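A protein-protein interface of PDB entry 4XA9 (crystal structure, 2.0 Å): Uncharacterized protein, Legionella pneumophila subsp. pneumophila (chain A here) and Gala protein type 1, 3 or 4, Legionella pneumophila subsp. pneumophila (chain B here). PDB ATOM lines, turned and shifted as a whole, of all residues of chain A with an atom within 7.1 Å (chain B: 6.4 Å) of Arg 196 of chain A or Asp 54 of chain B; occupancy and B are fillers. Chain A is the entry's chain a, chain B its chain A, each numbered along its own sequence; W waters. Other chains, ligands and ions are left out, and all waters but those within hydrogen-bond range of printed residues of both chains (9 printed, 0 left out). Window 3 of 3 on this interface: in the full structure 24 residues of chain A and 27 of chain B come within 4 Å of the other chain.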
ATOM      1  N   LYS A 189      11.499  16.080   0.755  1.00  0.00           N
ATOM      2  CA  LYS A 189      12.390  15.554   1.780  1.00  0.00           C
ATOM      3  C   LYS A 189      13.764  15.187   1.243  1.00  0.00           C
ATOM      4  O   LYS A 189      14.743  15.228   1.981  1.00  0.00           O
ATOM      5  CB  LYS A 189      11.764  14.332   2.461  1.00  0.00           C
ATOM      6  CG  LYS A 189      11.598  13.107   1.578  1.00  0.00           C
ATOM      7  CD  LYS A 189      11.089  11.929   2.402  1.00  0.00           C
ATOM      8  CE  LYS A 189      10.990  10.658   1.575  1.00  0.00           C
ATOM      9  NZ  LYS A 189      10.027  10.785   0.443  1.00  0.00           N
ATOM     10  N   GLU A 190      13.842  14.840  -0.040  1.00  0.00           N
ATOM     11  CA  GLU A 190      15.101  14.388  -0.618  1.00  0.00           C
ATOM     12  C   GLU A 190      16.133  15.510  -0.656  1.00  0.00           C
ATOM     13  O   GLU A 190      17.338  15.260  -0.675  1.00  0.00           O
ATOM     14  CB  GLU A 190      14.886  13.822  -2.025  1.00  0.00           C
ATOM     15  CG  GLU A 190      14.167  12.472  -2.060  1.00  0.00           C
ATOM     16  CD  GLU A 190      12.658  12.574  -1.877  1.00  0.00           C
ATOM     17  OE1 GLU A 190      12.102  13.693  -1.946  1.00  0.00           O
ATOM     18  OE2 GLU A 190      12.024  11.518  -1.669  1.00  0.00           O
ATOM     19  N   PHE A 192      16.068  17.977   1.678  1.00  0.00           N
ATOM     20  CA  PHE A 192      16.049  18.549   3.030  1.00  0.00           C
ATOM     21  C   PHE A 192      17.351  18.318   3.797  1.00  0.00           C
ATOM     22  O   PHE A 192      17.831  17.190   3.909  1.00  0.00           O
ATOM     23  CB  PHE A 192      14.851  17.974   3.807  1.00  0.00           C
ATOM     24  CG  PHE A 192      14.722  18.481   5.221  1.00  0.00           C
ATOM     25  CD1 PHE A 192      14.977  19.809   5.538  1.00  0.00           C
ATOM     26  CD2 PHE A 192      14.312  17.626   6.231  1.00  0.00           C
ATOM     27  CE1 PHE A 192      14.848  20.260   6.836  1.00  0.00           C
ATOM     28  CE2 PHE A 192      14.173  18.073   7.528  1.00  0.00           C
ATOM     29  CZ  PHE A 192      14.443  19.392   7.834  1.00  0.00           C
ATOM     30  N   ALA A 193      17.908  19.402   4.331  1.00  0.00           N
ATOM     31  CA  ALA A 193      19.151  19.361   5.091  1.00  0.00           C
ATOM     32  C   ALA A 193      19.125  18.342   6.230  1.00  0.00           C
ATOM     33  O   ALA A 193      20.142  17.714   6.518  1.00  0.00           O
ATOM     34  CB  ALA A 193      19.473  20.744   5.646  1.00  0.00           C
ATOM     35  N   TYR A 194      17.973  18.172   6.878  1.00  0.00           N
ATOM     36  CA  TYR A 194      17.901  17.245   8.006  1.00  0.00           C
ATOM     37  C   TYR A 194      17.068  16.017   7.691  1.00  0.00           C
ATOM     38  O   TYR A 194      16.433  15.428   8.570  1.00  0.00           O
ATOM     39  CB  TYR A 194      17.377  17.963   9.257  1.00  0.00           C
ATOM     40  CG  TYR A 194      18.492  18.704   9.947  1.00  0.00           C
ATOM     41  CD1 TYR A 194      18.867  19.978   9.531  1.00  0.00           C
ATOM     42  CD2 TYR A 194      19.218  18.106  10.967  1.00  0.00           C
ATOM     43  CE1 TYR A 194      19.914  20.646  10.134  1.00  0.00           C
ATOM     44  CE2 TYR A 194      20.267  18.768  11.577  1.00  0.00           C
ATOM     45  CZ  TYR A 194      20.611  20.034  11.155  1.00  0.00           C
ATOM     46  OH  TYR A 194      21.652  20.693  11.764  1.00  0.00           O
ATOM     47  N   ASN A 195      17.125  15.603   6.431  1.00  0.00           N
ATOM     48  CA  ASN A 195      16.438  14.402   5.987  1.00  0.00           C
ATOM     49  C   ASN A 195      16.846  13.150   6.775  1.00  0.00           C
ATOM     50  O   ASN A 195      16.055  12.221   6.922  1.00  0.00           O
ATOM     51  CB  ASN A 195      16.696  14.174   4.496  1.00  0.00           C
ATOM     52  CG  ASN A 195      15.831  13.071   3.924  1.00  0.00           C
ATOM     53  OD1 ASN A 195      14.702  12.867   4.368  1.00  0.00           O
ATOM     54  ND2 ASN A 195      16.357  12.346   2.947  1.00  0.00           N
ATOM     55  N   ARG A 196      18.076  13.130   7.284  1.00  0.00           N
ATOM     56  CA  ARG A 196      18.592  11.957   7.987  1.00  0.00           C
ATOM     57  C   ARG A 196      18.053  11.831   9.407  1.00  0.00           C
ATOM     58  O   ARG A 196      18.328  10.847  10.093  1.00  0.00           O
ATOM     59  CB  ARG A 196      20.125  11.981   8.033  1.00  0.00           C
ATOM     60  CG  ARG A 196      20.810  11.827   6.678  1.00  0.00           C
ATOM     61  CD  ARG A 196      20.572  10.449   6.076  1.00  0.00           C
ATOM     62  NE  ARG A 196      21.167  10.345   4.748  1.00  0.00           N
ATOM     63  CZ  ARG A 196      21.126   9.251   3.997  1.00  0.00           C
ATOM     64  NH1 ARG A 196      20.522   8.161   4.451  1.00  0.00           N
ATOM     65  NH2 ARG A 196      21.687   9.247   2.796  1.00  0.00           N
ATOM     66  N   SER A 197      17.298  12.825   9.864  1.00  0.00           N
ATOM     67  CA  SER A 197      16.687  12.733  11.185  1.00  0.00           C
ATOM     68  C   SER A 197      15.184  13.002  11.122  1.00  0.00           C
ATOM     69  O   SER A 197      14.524  13.153  12.153  1.00  0.00           O
ATOM     70  CB  SER A 197      17.355  13.711  12.152  1.00  0.00           C
ATOM     71  OG  SER A 197      17.173  15.045  11.711  1.00  0.00           O
ATOM     72  N   LEU A 198      14.647  13.052   9.907  1.00  0.00           N
ATOM     73  CA  LEU A 198      13.240  13.383   9.708  1.00  0.00           C
ATOM     74  C   LEU A 198      12.286  12.393  10.395  1.00  0.00           C
ATOM     75  O   LEU A 198      11.424  12.797  11.175  1.00  0.00           O
ATOM     76  CB  LEU A 198      12.934  13.456   8.217  1.00  0.00           C
ATOM     77  CG  LEU A 198      11.511  13.858   7.840  1.00  0.00           C
ATOM     78  CD1 LEU A 198      11.119  15.169   8.514  1.00  0.00           C
ATOM     79  CD2 LEU A 198      11.402  13.964   6.330  1.00  0.00           C
ATOM     80  N   PHE A 199      12.456  11.105  10.111  1.00  0.00           N
ATOM     81  CA  PHE A 199      11.581  10.064  10.656  1.00  0.00           C
ATOM     82  C   PHE A 199      12.302   9.234  11.715  1.00  0.00           C
ATOM     83  O   PHE A 199      13.511   9.030  11.618  1.00  0.00           O
ATOM     84  CB  PHE A 199      11.081   9.135   9.544  1.00  0.00           C
ATOM     85  CG  PHE A 199      10.457   9.849   8.386  1.00  0.00           C
ATOM     86  CD1 PHE A 199       9.211  10.439   8.508  1.00  0.00           C
ATOM     87  CD2 PHE A 199      11.107   9.908   7.165  1.00  0.00           C
ATOM     88  CE1 PHE A 199       8.627  11.089   7.433  1.00  0.00           C
ATOM     89  CE2 PHE A 199      10.532  10.555   6.087  1.00  0.00           C
ATOM     90  CZ  PHE A 199       9.286  11.147   6.220  1.00  0.00           C
ATOM     91  N   LEU B  25      25.815  16.310  -2.816  1.00  0.00           N
ATOM     92  CA  LEU B  25      25.984  15.925  -4.214  1.00  0.00           C
ATOM     93  C   LEU B  25      25.398  14.542  -4.487  1.00  0.00           C
ATOM     94  O   LEU B  25      25.575  13.996  -5.572  1.00  0.00           O
ATOM     95  CB  LEU B  25      27.470  15.954  -4.608  1.00  0.00           C
ATOM     96  CG  LEU B  25      28.135  17.332  -4.638  1.00  0.00           C
ATOM     97  CD1 LEU B  25      29.604  17.224  -5.026  1.00  0.00           C
ATOM     98  CD2 LEU B  25      27.399  18.257  -5.599  1.00  0.00           C
ATOM     99  N   ASN B  26      24.690  13.991  -3.504  1.00  0.00           N
ATOM    100  CA  ASN B  26      24.138  12.637  -3.594  1.00  0.00           C
ATOM    101  C   ASN B  26      25.186  11.595  -4.003  1.00  0.00           C
ATOM    102  O   ASN B  26      24.895  10.676  -4.764  1.00  0.00           O
ATOM    103  CB  ASN B  26      22.959  12.600  -4.574  1.00  0.00           C
ATOM    104  CG  ASN B  26      21.760  13.389  -4.071  1.00  0.00           C
ATOM    105  OD1 ASN B  26      21.032  12.934  -3.190  1.00  0.00           O
ATOM    106  ND2 ASN B  26      21.554  14.572  -4.629  1.00  0.00           N
ATOM    107  N   LEU B  27      26.403  11.739  -3.491  1.00  0.00           N
ATOM    108  CA  LEU B  27      27.464  10.779  -3.792  1.00  0.00           C
ATOM    109  C   LEU B  27      27.149   9.405  -3.219  1.00  0.00           C
ATOM    110  O   LEU B  27      26.516   9.284  -2.164  1.00  0.00           O
ATOM    111  CB  LEU B  27      28.809  11.261  -3.255  1.00  0.00           C
ATOM    112  CG  LEU B  27      29.290  12.636  -3.717  1.00  0.00           C
ATOM    113  CD1 LEU B  27      30.693  12.887  -3.190  1.00  0.00           C
ATOM    114  CD2 LEU B  27      29.244  12.744  -5.237  1.00  0.00           C
ATOM    115  N   ARG B  28      27.587   8.367  -3.923  1.00  0.00           N
ATOM    116  CA  ARG B  28      27.380   7.009  -3.459  1.00  0.00           C
ATOM    117  C   ARG B  28      28.700   6.292  -3.299  1.00  0.00           C
ATOM    118  O   ARG B  28      29.766   6.857  -3.573  1.00  0.00           O
ATOM    119  CB  ARG B  28      26.469   6.242  -4.416  1.00  0.00           C
ATOM    120  CG  ARG B  28      25.062   6.819  -4.485  1.00  0.00           C
ATOM    121  CD  ARG B  28      24.095   5.858  -5.144  1.00  0.00           C
ATOM    122  NE  ARG B  28      24.377   5.667  -6.566  1.00  0.00           N
ATOM    123  CZ  ARG B  28      23.747   6.307  -7.548  1.00  0.00           C
ATOM    124  NH1 ARG B  28      22.789   7.182  -7.266  1.00  0.00           N
ATOM    125  NH2 ARG B  28      24.071   6.067  -8.812  1.00  0.00           N
ATOM    126  N   ASP B  29      28.625   5.044  -2.856  1.00  0.00           N
ATOM    127  CA  ASP B  29      29.826   4.265  -2.607  1.00  0.00           C
ATOM    128  C   ASP B  29      30.720   4.170  -3.838  1.00  0.00           C
ATOM    129  O   ASP B  29      31.938   4.245  -3.716  1.00  0.00           O
ATOM    130  CB  ASP B  29      29.459   2.868  -2.123  1.00  0.00           C
ATOM    131  CG  ASP B  29      28.727   2.890  -0.803  1.00  0.00           C
ATOM    132  OD1 ASP B  29      28.851   3.890  -0.062  1.00  0.00           O
ATOM    133  OD2 ASP B  29      28.023   1.906  -0.504  1.00  0.00           O
ATOM    134  N   LEU B  50      32.567  15.345   3.188  1.00  0.00           N
ATOM    135  CA  LEU B  50      31.679  14.487   2.406  1.00  0.00           C
ATOM    136  C   LEU B  50      30.265  14.479   2.973  1.00  0.00           C
ATOM    137  O   LEU B  50      29.493  13.560   2.710  1.00  0.00           O
ATOM    138  CB  LEU B  50      32.208  13.054   2.361  1.00  0.00           C
ATOM    139  CG  LEU B  50      33.558  12.821   1.693  1.00  0.00           C
ATOM    140  CD1 LEU B  50      33.918  11.345   1.745  1.00  0.00           C
ATOM    141  CD2 LEU B  50      33.528  13.313   0.257  1.00  0.00           C
ATOM    142  N   HIS B  52      26.316  15.089   4.048  1.00  0.00           N
ATOM    143  CA  HIS B  52      25.057  15.192   3.316  1.00  0.00           C
ATOM    144  C   HIS B  52      25.139  14.510   1.943  1.00  0.00           C
ATOM    145  O   HIS B  52      24.906  15.126   0.905  1.00  0.00           O
ATOM    146  CB  HIS B  52      24.640  16.657   3.157  1.00  0.00           C
ATOM    147  CG  HIS B  52      24.421  17.372   4.459  1.00  0.00           C
ATOM    148  ND1 HIS B  52      23.245  17.276   5.174  1.00  0.00           N
ATOM    149  CD2 HIS B  52      25.214  18.222   5.157  1.00  0.00           C
ATOM    150  CE1 HIS B  52      23.330  18.021   6.262  1.00  0.00           C
ATOM    151  NE2 HIS B  52      24.512  18.610   6.274  1.00  0.00           N
ATOM    152  N   ASN B  53      25.482  13.229   1.957  1.00  0.00           N
ATOM    153  CA  ASN B  53      25.489  12.423   0.750  1.00  0.00           C
ATOM    154  C   ASN B  53      24.837  11.085   1.054  1.00  0.00           C
ATOM    155  O   ASN B  53      24.117  10.970   2.050  1.00  0.00           O
ATOM    156  CB  ASN B  53      26.913  12.263   0.222  1.00  0.00           C
ATOM    157  CG  ASN B  53      27.401  13.504  -0.496  1.00  0.00           C
ATOM    158  OD1 ASN B  53      26.786  13.944  -1.467  1.00  0.00           O
ATOM    159  ND2 ASN B  53      28.494  14.089  -0.011  1.00  0.00           N
ATOM    160  N   ASP B  54      25.086  10.077   0.221  1.00  0.00           N
ATOM    161  CA  ASP B  54      24.417   8.784   0.369  1.00  0.00           C
ATOM    162  C   ASP B  54      25.410   7.653   0.554  1.00  0.00           C
ATOM    163  O   ASP B  54      25.192   6.537   0.086  1.00  0.00           O
ATOM    164  CB  ASP B  54      23.537   8.496  -0.849  1.00  0.00           C
ATOM    165  CG  ASP B  54      22.469   9.548  -1.059  1.00  0.00           C
ATOM    166  OD1 ASP B  54      21.897  10.023  -0.057  1.00  0.00           O
ATOM    167  OD2 ASP B  54      22.210   9.907  -2.229  1.00  0.00           O
ATOM    168  N   ILE B  55      26.512   7.946   1.225  1.00  0.00           N
ATOM    169  CA  ILE B  55      27.579   6.972   1.403  1.00  0.00           C
ATOM    170  C   ILE B  55      27.203   5.940   2.464  1.00  0.00           C
ATOM    171  O   ILE B  55      26.608   6.282   3.487  1.00  0.00           O
ATOM    172  CB  ILE B  55      28.890   7.686   1.781  1.00  0.00           C
ATOM    173  CG1 ILE B  55      29.238   8.723   0.707  1.00  0.00           C
ATOM    174  CG2 ILE B  55      30.026   6.693   1.985  1.00  0.00           C
ATOM    175  CD1 ILE B  55      30.402   9.619   1.067  1.00  0.00           C
ATOM    176  N   THR B  56      27.534   4.675   2.211  1.00  0.00           N
ATOM    177  CA  THR B  56      27.282   3.608   3.173  1.00  0.00           C
ATOM    178  C   THR B  56      28.604   3.067   3.696  1.00  0.00           C
ATOM    179  O   THR B  56      29.661   3.615   3.394  1.00  0.00           O
ATOM    180  CB  THR B  56      26.479   2.444   2.560  1.00  0.00           C
ATOM    181  OG1 THR B  56      27.333   1.672   1.704  1.00  0.00           O
ATOM    182  CG2 THR B  56      25.280   2.962   1.769  1.00  0.00           C
ATOM    183  N   HIS B  76      25.790  13.086   8.129  1.00  0.00           N
ATOM    184  CA  HIS B  76      24.596  13.027   7.284  1.00  0.00           C
ATOM    185  C   HIS B  76      24.793  12.140   6.062  1.00  0.00           C
ATOM    186  O   HIS B  76      24.507  12.535   4.927  1.00  0.00           O
ATOM    187  CB  HIS B  76      24.174  14.431   6.853  1.00  0.00           C
ATOM    188  CG  HIS B  76      23.790  15.315   7.996  1.00  0.00           C
ATOM    189  ND1 HIS B  76      22.505  15.371   8.492  1.00  0.00           N
ATOM    190  CD2 HIS B  76      24.520  16.175   8.745  1.00  0.00           C
ATOM    191  CE1 HIS B  76      22.461  16.228   9.496  1.00  0.00           C
ATOM    192  NE2 HIS B  76      23.670  16.733   9.669  1.00  0.00           N
ATOM    193  N   ASN B  77      25.306  10.942   6.313  1.00  0.00           N
ATOM    194  CA  ASN B  77      25.311   9.873   5.325  1.00  0.00           C
ATOM    195  C   ASN B  77      24.585   8.664   5.912  1.00  0.00           C
ATOM    196  O   ASN B  77      23.709   8.827   6.753  1.00  0.00           O
ATOM    197  CB  ASN B  77      26.737   9.527   4.905  1.00  0.00           C
ATOM    198  CG  ASN B  77      27.306  10.533   3.915  1.00  0.00           C
ATOM    199  OD1 ASN B  77      27.117  10.401   2.708  1.00  0.00           O
ATOM    200  ND2 ASN B  77      28.009  11.540   4.425  1.00  0.00           N
ATOM    201  N   ASN B  78      24.954   7.460   5.486  1.00  0.00           N
ATOM    202  CA  ASN B  78      24.316   6.251   6.004  1.00  0.00           C
ATOM    203  C   ASN B  78      25.334   5.153   6.292  1.00  0.00           C
ATOM    204  O   ASN B  78      25.144   4.007   5.883  1.00  0.00           O
ATOM    205  CB  ASN B  78      23.267   5.743   5.005  1.00  0.00           C
ATOM    206  CG  ASN B  78      22.394   4.632   5.574  1.00  0.00           C
ATOM    207  OD1 ASN B  78      22.083   4.611   6.766  1.00  0.00           O
ATOM    208  ND2 ASN B  78      22.021   3.685   4.719  1.00  0.00           N
ATOM    209  N   PHE B 100      24.865  12.022  12.619  1.00  0.00           N
ATOM    210  CA  PHE B 100      23.725  11.648  11.780  1.00  0.00           C
ATOM    211  C   PHE B 100      24.049  10.512  10.812  1.00  0.00           C
ATOM    212  O   PHE B 100      23.887  10.656   9.598  1.00  0.00           O
ATOM    213  CB  PHE B 100      23.218  12.863  10.999  1.00  0.00           C
ATOM    214  CG  PHE B 100      22.689  13.966  11.877  1.00  0.00           C
ATOM    215  CD1 PHE B 100      23.543  14.927  12.401  1.00  0.00           C
ATOM    216  CD2 PHE B 100      21.338  14.030  12.190  1.00  0.00           C
ATOM    217  CE1 PHE B 100      23.053  15.944  13.223  1.00  0.00           C
ATOM    218  CE2 PHE B 100      20.841  15.040  13.010  1.00  0.00           C
ATOM    219  CZ  PHE B 100      21.701  15.997  13.527  1.00  0.00           C
ATOM    220  N   ASN B 101      24.504   9.388  11.354  1.00  0.00           N
ATOM    221  CA  ASN B 101      24.846   8.226  10.529  1.00  0.00           C
ATOM    222  C   ASN B 101      24.321   6.915  11.101  1.00  0.00           C
ATOM    223  O   ASN B 101      24.639   5.846  10.589  1.00  0.00           O
ATOM    224  CB  ASN B 101      26.363   8.115  10.349  1.00  0.00           C
ATOM    225  CG  ASN B 101      26.849   8.789   9.092  1.00  0.00           C
ATOM    226  OD1 ASN B 101      26.670   8.267   7.988  1.00  0.00           O
ATOM    227  ND2 ASN B 101      27.497   9.935   9.247  1.00  0.00           N
ATOM    228  N   GLU B 102      23.529   7.009  12.165  1.00  0.00           N
ATOM    229  CA  GLU B 102      23.024   5.836  12.877  1.00  0.00           C
ATOM    230  C   GLU B 102      24.129   4.850  13.259  1.00  0.00           C
ATOM    231  O   GLU B 102      23.942   3.637  13.144  1.00  0.00           O
ATOM    232  CB  GLU B 102      21.970   5.117  12.034  1.00  0.00           C
ATOM    233  CG  GLU B 102      20.896   6.028  11.463  1.00  0.00           C
ATOM    234  CD  GLU B 102      19.797   5.263  10.740  1.00  0.00           C
ATOM    235  OE1 GLU B 102      19.721   4.025  10.895  1.00  0.00           O
ATOM    236  OE2 GLU B 102      19.008   5.901  10.008  1.00  0.00           O
ATOM    237  N   TYR B 124      23.510  12.981  17.193  1.00  0.00           N
ATOM    238  CA  TYR B 124      22.376  12.175  16.719  1.00  0.00           C
ATOM    239  C   TYR B 124      22.785  10.858  16.054  1.00  0.00           C
ATOM    240  O   TYR B 124      22.746  10.731  14.837  1.00  0.00           O
ATOM    241  CB  TYR B 124      21.510  12.989  15.748  1.00  0.00           C
ATOM    242  CG  TYR B 124      20.141  12.379  15.540  1.00  0.00           C
ATOM    243  CD1 TYR B 124      19.171  12.464  16.533  1.00  0.00           C
ATOM    244  CD2 TYR B 124      19.822  11.703  14.366  1.00  0.00           C
ATOM    245  CE1 TYR B 124      17.920  11.898  16.364  1.00  0.00           C
ATOM    246  CE2 TYR B 124      18.568  11.131  14.185  1.00  0.00           C
ATOM    247  CZ  TYR B 124      17.624  11.233  15.190  1.00  0.00           C
ATOM    248  OH  TYR B 124      16.375  10.672  15.027  1.00  0.00           O
ATOM    249  N   LYS B 126      21.961   7.641  17.789  1.00  0.00           N
ATOM    250  CA  LYS B 126      21.368   6.623  18.662  1.00  0.00           C
ATOM    251  C   LYS B 126      22.382   6.083  19.669  1.00  0.00           C
ATOM    252  O   LYS B 126      22.332   4.912  20.051  1.00  0.00           O
ATOM    253  CB  LYS B 126      20.780   5.471  17.839  1.00  0.00           C
ATOM    254  CG  LYS B 126      19.735   5.915  16.827  1.00  0.00           C
ATOM    255  CD  LYS B 126      19.184   4.741  16.022  1.00  0.00           C
ATOM    256  CE  LYS B 126      19.128   5.073  14.529  1.00  0.00           C
ATOM    257  NZ  LYS B 126      19.288   6.539  14.252  1.00  0.00           N
HETATM  258  O   HOH W   1      22.242  12.782   3.202  1.00  0.00           O
HETATM  259  O   HOH W   2      19.012  13.011  -0.871  1.00  0.00           O
HETATM  260  O   HOH W   3      15.725   9.399  12.824  1.00  0.00           O
HETATM  261  O   HOH W   4      19.201   9.796   0.558  1.00  0.00           O
HETATM  262  O   HOH W   5      20.366  15.120   6.802  1.00  0.00           O
HETATM  263  O   HOH W   6      13.322  11.236  13.884  1.00  0.00           O
HETATM  264  O   HOH W   7      24.217  19.018  11.153  1.00  0.00           O
HETATM  265  O   HOH W   8      17.452   7.838   9.800  1.00  0.00           O
HETATM  266  O   HOH W   9      19.741   7.073   7.304  1.00  0.00           O
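Among the printed residues, pairs that only touch across the chains: Ala 193 of chain A with His 76 of chain B (3.9 Å), Tyr 194 of chain A with His 76 of chain B (3.9 Å), Tyr 194 of chain A with Phe 100 of chain B (3.7 Å), Arg 196 of chain A with His 76 of chain B (3.998 Å), Arg 196 of chain A with Asn 77 of chain B (3.6 Å), Arg 196 of chain A with Asn 78 of chain B (3.7 Å), Ser 197 of chain A with Phe 100 of chain B (3.8 Å) and Ser 197 of chain A with Tyr 124 of chain B (3.5 Å).
Glu 190 of chain A touches none of the printed residues of chain B. Printed residues of chain B within 4 Å of Tyr 194 of chain A: His 76 and Phe 100. Of the printed residues of chain B, Arg 196 of chain A touches Asn 53, Asp 54, His 76, Asn 77 and Asn 78. Of the printed residues of chain B, Ser 197 of chain A touches Phe 100 and Tyr 124. Of the printed residues of chain A, Asn 53 of chain B touches Arg 196. Of the printed residues of chain A, Asn 77 of chain B touches Arg 196 (3.6 Å). The nearest printed residue of chain B that does not touch Arg 196 of chain A is Tyr 124 of chain B (4.1 Å). The nearest residue of chain A that does not touch Asp 54 of chain B is Asn 195 of chain A (6.7 Å).
The backbone carbonyl oxygen of Ala 193 of chain A lies close to a ring nitrogen (ND1) of His 52 of chain B, at 3.4 Å. The backbone carbonyl oxygen (O) of Asn 53 of chain B sits at hydrogen-bond distance from the guanidinium group (NH2) of Arg 196 of chain A (3.1 Å). OD1 of Asp 54 of chain B lies within salt-bridge range of NH2 of Arg 196 of chain A (3.0 Å).
The backbone NH of Leu 25 of chain B sits at hydrogen-bond distance from the side-chain amide oxygen of Asn 53 of chain B (2.9 Å). The backbone NH (N) of Asn 26 of chain B lies within hydrogen-bond range of the side-chain amide oxygen (OD1) of Asn 53 of chain B, 2.9 Å away. The side-chain carboxylate (OD2) of Asp 54 of chain B sits close to the side-chain amide oxygen (OD1) of Asn 26 of chain B (3.4 Å). The backbone carbonyl oxygen (O) of Leu 50 of chain B sits at hydrogen-bond distance from the side-chain amide nitrogen (ND2) of Asn 53 of chain B, 2.9 Å away. N of Asn 53 of chain B lies within hydrogen-bond range of O of His 76 of chain B. The backbone carbonyl oxygen (O) of Ile 55 of chain B sits at hydrogen-bond distance from the backbone NH (N) of Asn 78 of chain B (2.8 Å).
Of the 10 printed residues of chain A, 4 touch a printed residue of chain B. Printed residues of chain A that touch a printed residue of chain B: Ala 193, Tyr 194, Arg 196 and Ser 197. Hydrophobic or aromatic side chains of chain A within 4 Å of the printed part of chain B: Tyr 194. Of the 19 printed residues of chain B, 8 touch a printed residue of chain A. Among the printed residues, Asp or Glu carboxylates within 4 Å of a Lys or Arg side-chain nitrogen of the other chain: Arg 196 of chain A with Asp 54 of chain B (3.0 Å).
Water W8 lies within hydrogen-bond range of OE2 of Glu 102 of chain B (2.5 Å) and O of Arg 196 of chain A (3.1 Å). Water W3 lies within hydrogen-bond range of O of Phe 199 of chain A (2.5 Å) and OH of Tyr 124 of chain B (2.6 Å). Water W5 lies within hydrogen-bond range of the backbone carbonyl oxygen of Ala 193 of chain A (2.6 Å), a ring nitrogen (ND1) of His 76 of chain B (2.7 Å), the backbone NH of Arg 196 of chain A (3.1 Å) and the backbone NH of Asn 195 of chain A (3.3 Å). Water W2 bridges O of Glu 190 of chain A (2.8 Å) and OD1 of Asn 26 of chain B (3.1 Å). Water W6 lies within hydrogen-bond range of O of Ser 197 of chain A (2.8 Å), O of Phe 199 of chain A (3.2 Å) and OH of Tyr 124 of chain B (3.3 Å). Water W1 lies within hydrogen-bond range of O of Asn 53 of chain B (2.9 Å), O of His 76 of chain B (2.9 Å) and NE of Arg 196 of chain A (3.1 Å).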
